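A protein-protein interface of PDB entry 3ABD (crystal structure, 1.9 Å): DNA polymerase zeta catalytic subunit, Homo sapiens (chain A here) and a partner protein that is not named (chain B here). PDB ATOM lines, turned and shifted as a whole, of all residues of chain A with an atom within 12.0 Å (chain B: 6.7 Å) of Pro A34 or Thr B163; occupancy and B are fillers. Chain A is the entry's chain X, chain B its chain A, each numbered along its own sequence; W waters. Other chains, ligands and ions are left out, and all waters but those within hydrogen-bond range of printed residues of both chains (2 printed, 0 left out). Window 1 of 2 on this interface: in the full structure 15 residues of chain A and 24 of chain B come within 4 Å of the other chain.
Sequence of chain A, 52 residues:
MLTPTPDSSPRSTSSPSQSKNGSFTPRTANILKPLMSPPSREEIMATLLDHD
Leu A32 touches Leu B165. Leu A32 touches Ile B188. Val B164 touches Lys A33 (O to CB, 3.6 Å). Trp B187 touches Lys A33. Pro A34 touches Tyr B79 (CB to OH, 3.4 Å). Pro A34 touches Phe B185. Pro A34 touches Trp B187. Met A36 touches Pro B186 (CE to CG, 3.7 Å). Ser A37 touches Tyr B79. Tyr B79 touches Pro A38 (OH to CD, 3.3 Å).
N of Val B102 sits at hydrogen-bond distance from O of Thr B163 (2.9 Å). The backbone carbonyl oxygen (O) of Tyr B79 sits at hydrogen-bond distance from the side-chain hydroxyl (OG1) of Thr B83 (2.8 Å). The backbone carbonyl oxygen (O) of Leu B165 lies within hydrogen-bond range of the backbone NH (N) of Val B100, 2.7 Å away.
Water W2 lies within hydrogen-bond range of OG1 of Thr B163 (2.7 Å) and O of Pro A34 (2.8 Å). Water W1 lies within hydrogen-bond range of O of Pro B186 (2.8 Å), N of Met A36 (3.0 Å) and N of Leu A35 (3.3 Å).
Printed residues of chain B within 4 Å of Pro A34: Tyr B79 (3.4 Å), Thr B163 (3.99 Å), Val B164 (3.1 Å), Phe B185 (3.7 Å), Pro B186 (3.6 Å) and Trp B187 (3.6 Å). Printed residues of chain B within 4 Å of Leu A35: Pro B186 and Ile B188. Pro A39 touches none of the printed residues of chain B. Arg A41 touches none of the printed residues of chain B. Of the printed residues of chain A, Tyr B79 touches Pro A34 (3.4 Å), Met A36 (2.6 Å), Ser A37 (3.4 Å) and Pro A38 (3.3 Å). No residue of chain A comes within 4 Å of Thr B83. No residue of chain A comes within 4 Å of Val B100. No residue of chain A comes within 4 Å of Val B101. No residue of chain A comes within 4 Å of Ile B103. No residue of chain A comes within 4 Å of Leu B104. Thr B161 touches none of the printed residues of chain A. Printed residues of chain A within 4 Å of Thr B163: Pro A34 (3.99 Å). Asp B194 touches just one residue of chain A: Lys A33 (2.8 Å).
Of the 18 printed residues of chain B, 11 touch a printed residue of chain A. Printed residues of chain B that touch a printed residue of chain A: Tyr B79, Phe B162, Thr B163, Val B164, Leu B165, Val B166, Phe B185, Pro B186, Trp B187, Ile B188 and Asp B194. Among the printed residues, Asp or Glu carboxylates within 4 Å of a Lys or Arg side-chain nitrogen of the other chain: Lys A33 with Asp B194.
The backbone carbonyl oxygen (O) of Pro B186 lies within hydrogen-bond range of the backbone NH (N) of Leu A35 (2.7 Å). N of Val B166 is in hydrogen-bond range of O of Leu A32. O of Asn A30 lies close to O of Val B166 (3.5 Å). The backbone NH (N) of Ile B188 lies within hydrogen-bond range of the backbone carbonyl oxygen (O) of Lys A33, at 2.8 Å. OD2 of Asp B194 lies within salt-bridge range of NZ of Lys A33, at 3.0 Å. The side-chain hydroxyl (OH) of Tyr B79 is in hydrogen-bond range of the backbone carbonyl oxygen (O) of Met A36 (2.6 Å).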
ATOM      1  N   ASN A  30      32.013  17.454  13.456  1.00  0.00           N
ATOM      2  CA  ASN A  30      30.676  17.526  12.884  1.00  0.00           C
ATOM      3  C   ASN A  30      29.918  16.198  12.934  1.00  0.00           C
ATOM      4  O   ASN A  30      29.076  15.933  12.076  1.00  0.00           O
ATOM      5  CB  ASN A  30      30.741  17.994  11.453  1.00  0.00           C
ATOM      6  CG  ASN A  30      31.265  19.398  11.327  1.00  0.00           C
ATOM      7  OD1 ASN A  30      31.407  20.114  12.318  1.00  0.00           O
ATOM      8  ND2 ASN A  30      31.560  19.806  10.100  1.00  0.00           N
ATOM      9  N   ILE A  31      30.233  15.385  13.934  1.00  0.00           N
ATOM     10  CA  ILE A  31      29.478  14.151  14.233  1.00  0.00           C
ATOM     11  C   ILE A  31      28.735  14.299  15.553  1.00  0.00           C
ATOM     12  O   ILE A  31      29.349  14.515  16.604  1.00  0.00           O
ATOM     13  CB  ILE A  31      30.415  12.929  14.298  1.00  0.00           C
ATOM     14  CG1 ILE A  31      31.317  12.908  13.049  1.00  0.00           C
ATOM     15  CG2 ILE A  31      29.577  11.642  14.399  1.00  0.00           C
ATOM     16  CD1 ILE A  31      32.352  11.828  13.057  1.00  0.00           C
ATOM     17  N   LEU A  32      27.413  14.236  15.478  1.00  0.00           N
ATOM     18  CA  LEU A  32      26.528  14.387  16.615  1.00  0.00           C
ATOM     19  C   LEU A  32      25.857  13.059  16.951  1.00  0.00           C
ATOM     20  O   LEU A  32      25.521  12.267  16.038  1.00  0.00           O
ATOM     21  CB  LEU A  32      25.433  15.351  16.257  1.00  0.00           C
ATOM     22  CG  LEU A  32      25.959  16.686  15.710  1.00  0.00           C
ATOM     23  CD1 LEU A  32      24.859  17.307  14.883  1.00  0.00           C
ATOM     24  CD2 LEU A  32      26.395  17.546  16.852  1.00  0.00           C
ATOM     25  N   LYS A  33      25.635  12.829  18.244  1.00  0.00           N
ATOM     26  CA  LYS A  33      24.792  11.701  18.675  1.00  0.00           C
ATOM     27  C   LYS A  33      23.792  12.146  19.754  1.00  0.00           C
ATOM     28  O   LYS A  33      24.012  13.170  20.391  1.00  0.00           O
ATOM     29  CB  LYS A  33      25.635  10.524  19.126  1.00  0.00           C
ATOM     30  CG  LYS A  33      26.183  10.566  20.513  1.00  0.00           C
ATOM     31  CD  LYS A  33      27.087   9.367  20.794  1.00  0.00           C
ATOM     32  CE  LYS A  33      27.319   9.101  22.286  1.00  0.00           C
ATOM     33  NZ  LYS A  33      28.067  10.219  22.866  1.00  0.00           N
ATOM     34  N   PRO A  34      22.693  11.405  19.925  1.00  0.00           N
ATOM     35  CA  PRO A  34      21.806  11.657  21.050  1.00  0.00           C
ATOM     36  C   PRO A  34      22.567  11.493  22.334  1.00  0.00           C
ATOM     37  O   PRO A  34      23.366  10.575  22.487  1.00  0.00           O
ATOM     38  CB  PRO A  34      20.747  10.589  20.930  1.00  0.00           C
ATOM     39  CG  PRO A  34      20.799  10.197  19.426  1.00  0.00           C
ATOM     40  CD  PRO A  34      22.208  10.316  19.058  1.00  0.00           C
ATOM     41  N   LEU A  35      22.311  12.405  23.271  1.00  0.00           N
ATOM     42  CA  LEU A  35      22.909  12.271  24.587  1.00  0.00           C
ATOM     43  C   LEU A  35      22.261  11.122  25.321  1.00  0.00           C
ATOM     44  O   LEU A  35      22.971  10.342  25.976  1.00  0.00           O
ATOM     45  CB  LEU A  35      22.797  13.576  25.393  1.00  0.00           C
ATOM     46  CG  LEU A  35      23.378  13.509  26.818  1.00  0.00           C
ATOM     47  CD1 LEU A  35      24.819  13.562  26.875  1.00  0.00           C
ATOM     48  CD2 LEU A  35      22.804  14.664  27.578  1.00  0.00           C
ATOM     49  N   MET A  36      20.945  10.981  25.235  1.00  0.00           N
ATOM     50  CA  MET A  36      20.258   9.840  25.883  1.00  0.00           C
ATOM     51  C   MET A  36      20.466   8.577  25.066  1.00  0.00           C
ATOM     52  O   MET A  36      20.531   8.657  23.841  1.00  0.00           O
ATOM     53  CB  MET A  36      18.751  10.022  25.920  1.00  0.00           C
ATOM     54  CG  MET A  36      18.280  11.326  26.013  1.00  0.00           C
ATOM     55  SD  MET A  36      18.444  11.723  27.751  1.00  0.00           S
ATOM     56  CE  MET A  36      19.977  12.628  27.621  1.00  0.00           C
ATOM     57  N   SER A  37      20.605   7.444  25.764  1.00  0.00           N
ATOM     58  CA  SER A  37      20.715   6.123  25.158  1.00  0.00           C
ATOM     59  C   SER A  37      19.336   5.537  24.950  1.00  0.00           C
ATOM     60  O   SER A  37      18.419   5.879  25.656  1.00  0.00           O
ATOM     61  CB  SER A  37      21.498   5.188  26.081  1.00  0.00           C
ATOM     62  OG  SER A  37      22.797   5.676  26.245  1.00  0.00           O
ATOM     63  N   PRO A  38      19.195   4.605  23.981  1.00  0.00           N
ATOM     64  CA  PRO A  38      17.934   3.874  23.838  1.00  0.00           C
ATOM     65  C   PRO A  38      17.701   2.963  25.042  1.00  0.00           C
ATOM     66  O   PRO A  38      18.649   2.669  25.768  1.00  0.00           O
ATOM     67  CB  PRO A  38      18.140   3.067  22.555  1.00  0.00           C
ATOM     68  CG  PRO A  38      19.594   3.028  22.352  1.00  0.00           C
ATOM     69  CD  PRO A  38      20.109   4.334  22.872  1.00  0.00           C
ATOM     70  N   PRO A  39      16.452   2.529  25.278  1.00  0.00           N
ATOM     71  CA  PRO A  39      16.299   1.581  26.416  1.00  0.00           C
ATOM     72  C   PRO A  39      17.178   0.334  26.233  1.00  0.00           C
ATOM     73  O   PRO A  39      17.322  -0.149  25.128  1.00  0.00           O
ATOM     74  CB  PRO A  39      14.813   1.236  26.396  1.00  0.00           C
ATOM     75  CG  PRO A  39      14.258   1.786  25.137  1.00  0.00           C
ATOM     76  CD  PRO A  39      15.174   2.845  24.632  1.00  0.00           C
ATOM     77  N   SER A  40      17.802  -0.184  27.288  1.00  0.00           N
ATOM     78  CA  SER A  40      18.576  -1.416  27.159  1.00  0.00           C
ATOM     79  C   SER A  40      17.635  -2.582  26.829  1.00  0.00           C
ATOM     80  O   SER A  40      16.500  -2.572  27.200  1.00  0.00           O
ATOM     81  CB  SER A  40      19.343  -1.761  28.453  1.00  0.00           C
ATOM     82  OG  SER A  40      18.468  -1.850  29.598  1.00  0.00           O
ATOM     83  N   ARG A  41      18.163  -3.575  26.128  1.00  0.00           N
ATOM     84  CA  ARG A  41      17.485  -4.828  25.898  1.00  0.00           C
ATOM     85  C   ARG A  41      17.083  -5.441  27.247  1.00  0.00           C
ATOM     86  O   ARG A  41      16.006  -6.015  27.373  1.00  0.00           O
ATOM     87  CB  ARG A  41      18.432  -5.745  25.144  1.00  0.00           C
ATOM     88  CG  ARG A  41      17.884  -7.090  24.723  1.00  0.00           C
ATOM     89  CD  ARG A  41      19.010  -7.962  24.203  1.00  0.00           C
ATOM     90  NE  ARG A  41      18.574  -9.316  23.875  1.00  0.00           N
ATOM     91  CZ  ARG A  41      18.471  -9.786  22.628  1.00  0.00           C
ATOM     92  NH1 ARG A  41      18.760  -9.019  21.589  1.00  0.00           N
ATOM     93  NH2 ARG A  41      18.060 -11.019  22.412  1.00  0.00           N
ATOM     94  N   TYR B  79      11.967   6.585  21.150  1.00  0.00           N
ATOM     95  CA  TYR B  79      13.386   6.965  21.021  1.00  0.00           C
ATOM     96  C   TYR B  79      13.802   7.220  19.583  1.00  0.00           C
ATOM     97  O   TYR B  79      14.398   8.290  19.239  1.00  0.00           O
ATOM     98  CB  TYR B  79      14.263   5.914  21.663  1.00  0.00           C
ATOM     99  CG  TYR B  79      15.711   6.300  21.709  1.00  0.00           C
ATOM    100  CD1 TYR B  79      16.227   7.064  22.753  1.00  0.00           C
ATOM    101  CD2 TYR B  79      16.539   5.980  20.682  1.00  0.00           C
ATOM    102  CE1 TYR B  79      17.548   7.476  22.744  1.00  0.00           C
ATOM    103  CE2 TYR B  79      17.857   6.350  20.698  1.00  0.00           C
ATOM    104  CZ  TYR B  79      18.343   7.090  21.742  1.00  0.00           C
ATOM    105  OH  TYR B  79      19.661   7.412  21.689  1.00  0.00           O
ATOM    106  N   THR B  83      14.711  10.760  17.739  1.00  0.00           N
ATOM    107  CA  THR B  83      16.005  10.902  17.072  1.00  0.00           C
ATOM    108  C   THR B  83      15.778  11.490  15.680  1.00  0.00           C
ATOM    109  O   THR B  83      16.412  12.505  15.294  1.00  0.00           O
ATOM    110  CB  THR B  83      16.766   9.550  17.074  1.00  0.00           C
ATOM    111  OG1 THR B  83      16.966   9.129  18.446  1.00  0.00           O
ATOM    112  CG2 THR B  83      18.064   9.669  16.336  1.00  0.00           C
ATOM    113  N   VAL B 100      24.234   7.443  10.452  1.00  0.00           N
ATOM    114  CA  VAL B 100      24.864   6.181  10.701  1.00  0.00           C
ATOM    115  C   VAL B 100      24.197   5.483  11.876  1.00  0.00           C
ATOM    116  O   VAL B 100      24.034   6.079  12.953  1.00  0.00           O
ATOM    117  CB  VAL B 100      26.369   6.326  10.968  1.00  0.00           C
ATOM    118  CG1 VAL B 100      26.988   4.955  11.099  1.00  0.00           C
ATOM    119  CG2 VAL B 100      27.058   7.201   9.908  1.00  0.00           C
ATOM    120  N   VAL B 101      23.766   4.260  11.678  1.00  0.00           N
ATOM    121  CA  VAL B 101      23.264   3.439  12.767  1.00  0.00           C
ATOM    122  C   VAL B 101      24.440   2.574  13.237  1.00  0.00           C
ATOM    123  O   VAL B 101      24.957   1.760  12.477  1.00  0.00           O
ATOM    124  CB  VAL B 101      22.100   2.513  12.368  1.00  0.00           C
ATOM    125  CG1 VAL B 101      21.652   1.734  13.495  1.00  0.00           C
ATOM    126  CG2 VAL B 101      20.928   3.278  11.758  1.00  0.00           C
ATOM    127  N   VAL B 102      24.848   2.769  14.473  1.00  0.00           N
ATOM    128  CA  VAL B 102      26.028   2.134  15.005  1.00  0.00           C
ATOM    129  C   VAL B 102      25.610   1.086  16.024  1.00  0.00           C
ATOM    130  O   VAL B 102      24.926   1.372  16.967  1.00  0.00           O
ATOM    131  CB  VAL B 102      26.938   3.153  15.698  1.00  0.00           C
ATOM    132  CG1 VAL B 102      28.181   2.455  16.264  1.00  0.00           C
ATOM    133  CG2 VAL B 102      27.361   4.207  14.702  1.00  0.00           C
ATOM    134  N   ILE B 103      26.052  -0.117  15.839  1.00  0.00           N
ATOM    135  CA  ILE B 103      25.823  -1.146  16.813  1.00  0.00           C
ATOM    136  C   ILE B 103      27.084  -1.296  17.669  1.00  0.00           C
ATOM    137  O   ILE B 103      28.204  -1.356  17.145  1.00  0.00           O
ATOM    138  CB  ILE B 103      25.478  -2.407  16.096  1.00  0.00           C
ATOM    139  CG1 ILE B 103      24.164  -2.142  15.325  1.00  0.00           C
ATOM    140  CG2 ILE B 103      25.301  -3.518  17.082  1.00  0.00           C
ATOM    141  CD1 ILE B 103      23.791  -3.156  14.496  1.00  0.00           C
ATOM    142  N   LEU B 104      26.906  -1.259  18.961  1.00  0.00           N
ATOM    143  CA  LEU B 104      27.946  -1.184  19.977  1.00  0.00           C
ATOM    144  C   LEU B 104      27.900  -2.430  20.842  1.00  0.00           C
ATOM    145  O   LEU B 104      26.825  -2.902  21.182  1.00  0.00           O
ATOM    146  CB  LEU B 104      27.657   0.031  20.908  1.00  0.00           C
ATOM    147  CG  LEU B 104      27.626   1.435  20.299  1.00  0.00           C
ATOM    148  CD1 LEU B 104      27.090   2.441  21.342  1.00  0.00           C
ATOM    149  CD2 LEU B 104      29.090   1.722  19.999  1.00  0.00           C
ATOM    150  N   THR B 161      24.113  -2.781  21.924  1.00  0.00           N
ATOM    151  CA  THR B 161      23.159  -1.705  21.920  1.00  0.00           C
ATOM    152  C   THR B 161      23.390  -0.924  20.627  1.00  0.00           C
ATOM    153  O   THR B 161      24.143  -1.358  19.761  1.00  0.00           O
ATOM    154  CB  THR B 161      23.393  -0.773  23.133  1.00  0.00           C
ATOM    155  OG1 THR B 161      24.714  -0.234  23.064  1.00  0.00           O
ATOM    156  CG2 THR B 161      23.332  -1.551  24.414  1.00  0.00           C
ATOM    157  N   PHE B 162      22.741   0.225  20.484  1.00  0.00           N
ATOM    158  CA  PHE B 162      22.902   1.048  19.270  1.00  0.00           C
ATOM    159  C   PHE B 162      22.861   2.521  19.615  1.00  0.00           C
ATOM    160  O   PHE B 162      22.414   2.935  20.683  1.00  0.00           O
ATOM    161  CB  PHE B 162      21.896   0.744  18.161  1.00  0.00           C
ATOM    162  CG  PHE B 162      20.533   1.402  18.344  1.00  0.00           C
ATOM    163  CD1 PHE B 162      19.631   0.911  19.288  1.00  0.00           C
ATOM    164  CD2 PHE B 162      20.167   2.512  17.609  1.00  0.00           C
ATOM    165  CE1 PHE B 162      18.397   1.539  19.502  1.00  0.00           C
ATOM    166  CE2 PHE B 162      18.858   3.105  17.785  1.00  0.00           C
ATOM    167  CZ  PHE B 162      18.020   2.611  18.753  1.00  0.00           C
ATOM    168  N   THR B 163      23.386   3.297  18.680  1.00  0.00           N
ATOM    169  CA  THR B 163      23.186   4.721  18.671  1.00  0.00           C
ATOM    170  C   THR B 163      23.061   5.153  17.219  1.00  0.00           C
ATOM    171  O   THR B 163      23.280   4.380  16.270  1.00  0.00           O
ATOM    172  CB  THR B 163      24.372   5.454  19.393  1.00  0.00           C
ATOM    173  OG1 THR B 163      24.071   6.827  19.573  1.00  0.00           O
ATOM    174  CG2 THR B 163      25.629   5.406  18.587  1.00  0.00           C
ATOM    175  N   VAL B 164      22.750   6.407  17.034  1.00  0.00           N
ATOM    176  CA  VAL B 164      22.693   6.992  15.706  1.00  0.00           C
ATOM    177  C   VAL B 164      23.644   8.154  15.679  1.00  0.00           C
ATOM    178  O   VAL B 164      23.633   8.989  16.593  1.00  0.00           O
ATOM    179  CB  VAL B 164      21.237   7.447  15.399  1.00  0.00           C
ATOM    180  CG1 VAL B 164      21.140   8.161  14.054  1.00  0.00           C
ATOM    181  CG2 VAL B 164      20.309   6.267  15.441  1.00  0.00           C
ATOM    182  N   LEU B 165      24.473   8.230  14.645  1.00  0.00           N
ATOM    183  CA  LEU B 165      25.382   9.331  14.523  1.00  0.00           C
ATOM    184  C   LEU B 165      24.966  10.082  13.276  1.00  0.00           C
ATOM    185  O   LEU B 165      24.616   9.481  12.253  1.00  0.00           O
ATOM    186  CB  LEU B 165      26.810   8.813  14.349  1.00  0.00           C
ATOM    187  CG  LEU B 165      27.403   8.065  15.548  1.00  0.00           C
ATOM    188  CD1 LEU B 165      28.850   7.617  15.222  1.00  0.00           C
ATOM    189  CD2 LEU B 165      27.400   8.972  16.693  1.00  0.00           C
ATOM    190  N   VAL B 166      25.031  11.389  13.355  1.00  0.00           N
ATOM    191  CA  VAL B 166      24.698  12.216  12.234  1.00  0.00           C
ATOM    192  C   VAL B 166      25.961  13.022  11.906  1.00  0.00           C
ATOM    193  O   VAL B 166      26.516  13.680  12.790  1.00  0.00           O
ATOM    194  CB  VAL B 166      23.512  13.144  12.574  1.00  0.00           C
ATOM    195  CG1 VAL B 166      23.247  14.192  11.443  1.00  0.00           C
ATOM    196  CG2 VAL B 166      22.287  12.355  12.784  1.00  0.00           C
ATOM    197  N   PHE B 185      15.392  16.332  23.984  1.00  0.00           N
ATOM    198  CA  PHE B 185      16.254  15.358  23.329  1.00  0.00           C
ATOM    199  C   PHE B 185      17.587  15.895  22.839  1.00  0.00           C
ATOM    200  O   PHE B 185      17.776  16.206  21.693  1.00  0.00           O
ATOM    201  CB  PHE B 185      15.482  14.667  22.230  1.00  0.00           C
ATOM    202  CG  PHE B 185      15.971  13.279  21.924  1.00  0.00           C
ATOM    203  CD1 PHE B 185      15.583  12.211  22.694  1.00  0.00           C
ATOM    204  CD2 PHE B 185      16.807  13.050  20.867  1.00  0.00           C
ATOM    205  CE1 PHE B 185      16.001  10.964  22.389  1.00  0.00           C
ATOM    206  CE2 PHE B 185      17.223  11.792  20.569  1.00  0.00           C
ATOM    207  CZ  PHE B 185      16.826  10.753  21.338  1.00  0.00           C
ATOM    208  N   PRO B 186      18.521  15.968  23.749  1.00  0.00           N
ATOM    209  CA  PRO B 186      19.774  16.699  23.581  1.00  0.00           C
ATOM    210  C   PRO B 186      20.821  15.879  22.824  1.00  0.00           C
ATOM    211  O   PRO B 186      20.974  14.690  23.075  1.00  0.00           O
ATOM    212  CB  PRO B 186      20.221  16.948  25.027  1.00  0.00           C
ATOM    213  CG  PRO B 186      19.632  15.821  25.797  1.00  0.00           C
ATOM    214  CD  PRO B 186      18.319  15.515  25.137  1.00  0.00           C
ATOM    215  N   TRP B 187      21.537  16.526  21.912  1.00  0.00           N
ATOM    216  CA  TRP B 187      22.579  15.863  21.139  1.00  0.00           C
ATOM    217  C   TRP B 187      23.901  16.364  21.642  1.00  0.00           C
ATOM    218  O   TRP B 187      24.002  17.512  22.147  1.00  0.00           O
ATOM    219  CB  TRP B 187      22.428  16.182  19.642  1.00  0.00           C
ATOM    220  CG  TRP B 187      21.249  15.545  19.050  1.00  0.00           C
ATOM    221  CD1 TRP B 187      19.933  15.793  19.350  1.00  0.00           C
ATOM    222  CD2 TRP B 187      21.254  14.505  18.078  1.00  0.00           C
ATOM    223  NE1 TRP B 187      19.121  14.999  18.574  1.00  0.00           N
ATOM    224  CE2 TRP B 187      19.911  14.196  17.787  1.00  0.00           C
ATOM    225  CE3 TRP B 187      22.258  13.864  17.364  1.00  0.00           C
ATOM    226  CZ2 TRP B 187      19.558  13.204  16.859  1.00  0.00           C
ATOM    227  CZ3 TRP B 187      21.907  12.882  16.451  1.00  0.00           C
ATOM    228  CH2 TRP B 187      20.559  12.581  16.198  1.00  0.00           C
ATOM    229  N   ILE B 188      24.898  15.514  21.531  1.00  0.00           N
ATOM    230  CA  ILE B 188      26.220  15.790  22.025  1.00  0.00           C
ATOM    231  C   ILE B 188      27.214  15.453  20.911  1.00  0.00           C
ATOM    232  O   ILE B 188      26.919  14.623  20.053  1.00  0.00           O
ATOM    233  CB  ILE B 188      26.487  14.992  23.345  1.00  0.00           C
ATOM    234  CG1 ILE B 188      27.850  15.296  23.952  1.00  0.00           C
ATOM    235  CG2 ILE B 188      26.388  13.482  23.126  1.00  0.00           C
ATOM    236  CD1 ILE B 188      28.005  14.711  25.429  1.00  0.00           C
ATOM    237  N   ASP B 194      32.917   6.410  20.267  1.00  0.00           N
ATOM    238  CA  ASP B 194      31.679   6.076  19.581  1.00  0.00           C
ATOM    239  C   ASP B 194      31.914   5.773  18.138  1.00  0.00           C
ATOM    240  O   ASP B 194      31.150   5.060  17.522  1.00  0.00           O
ATOM    241  CB  ASP B 194      30.719   7.224  19.689  1.00  0.00           C
ATOM    242  CG  ASP B 194      30.063   7.268  21.000  1.00  0.00           C
ATOM    243  OD1 ASP B 194      29.658   6.189  21.468  1.00  0.00           O
ATOM    244  OD2 ASP B 194      29.970   8.347  21.567  1.00  0.00           O
HETATM  245  O   HOH W   1      19.073  12.697  23.595  1.00  0.00           O
HETATM  246  O   HOH W   2      23.738   7.858  22.082  1.00  0.00           O
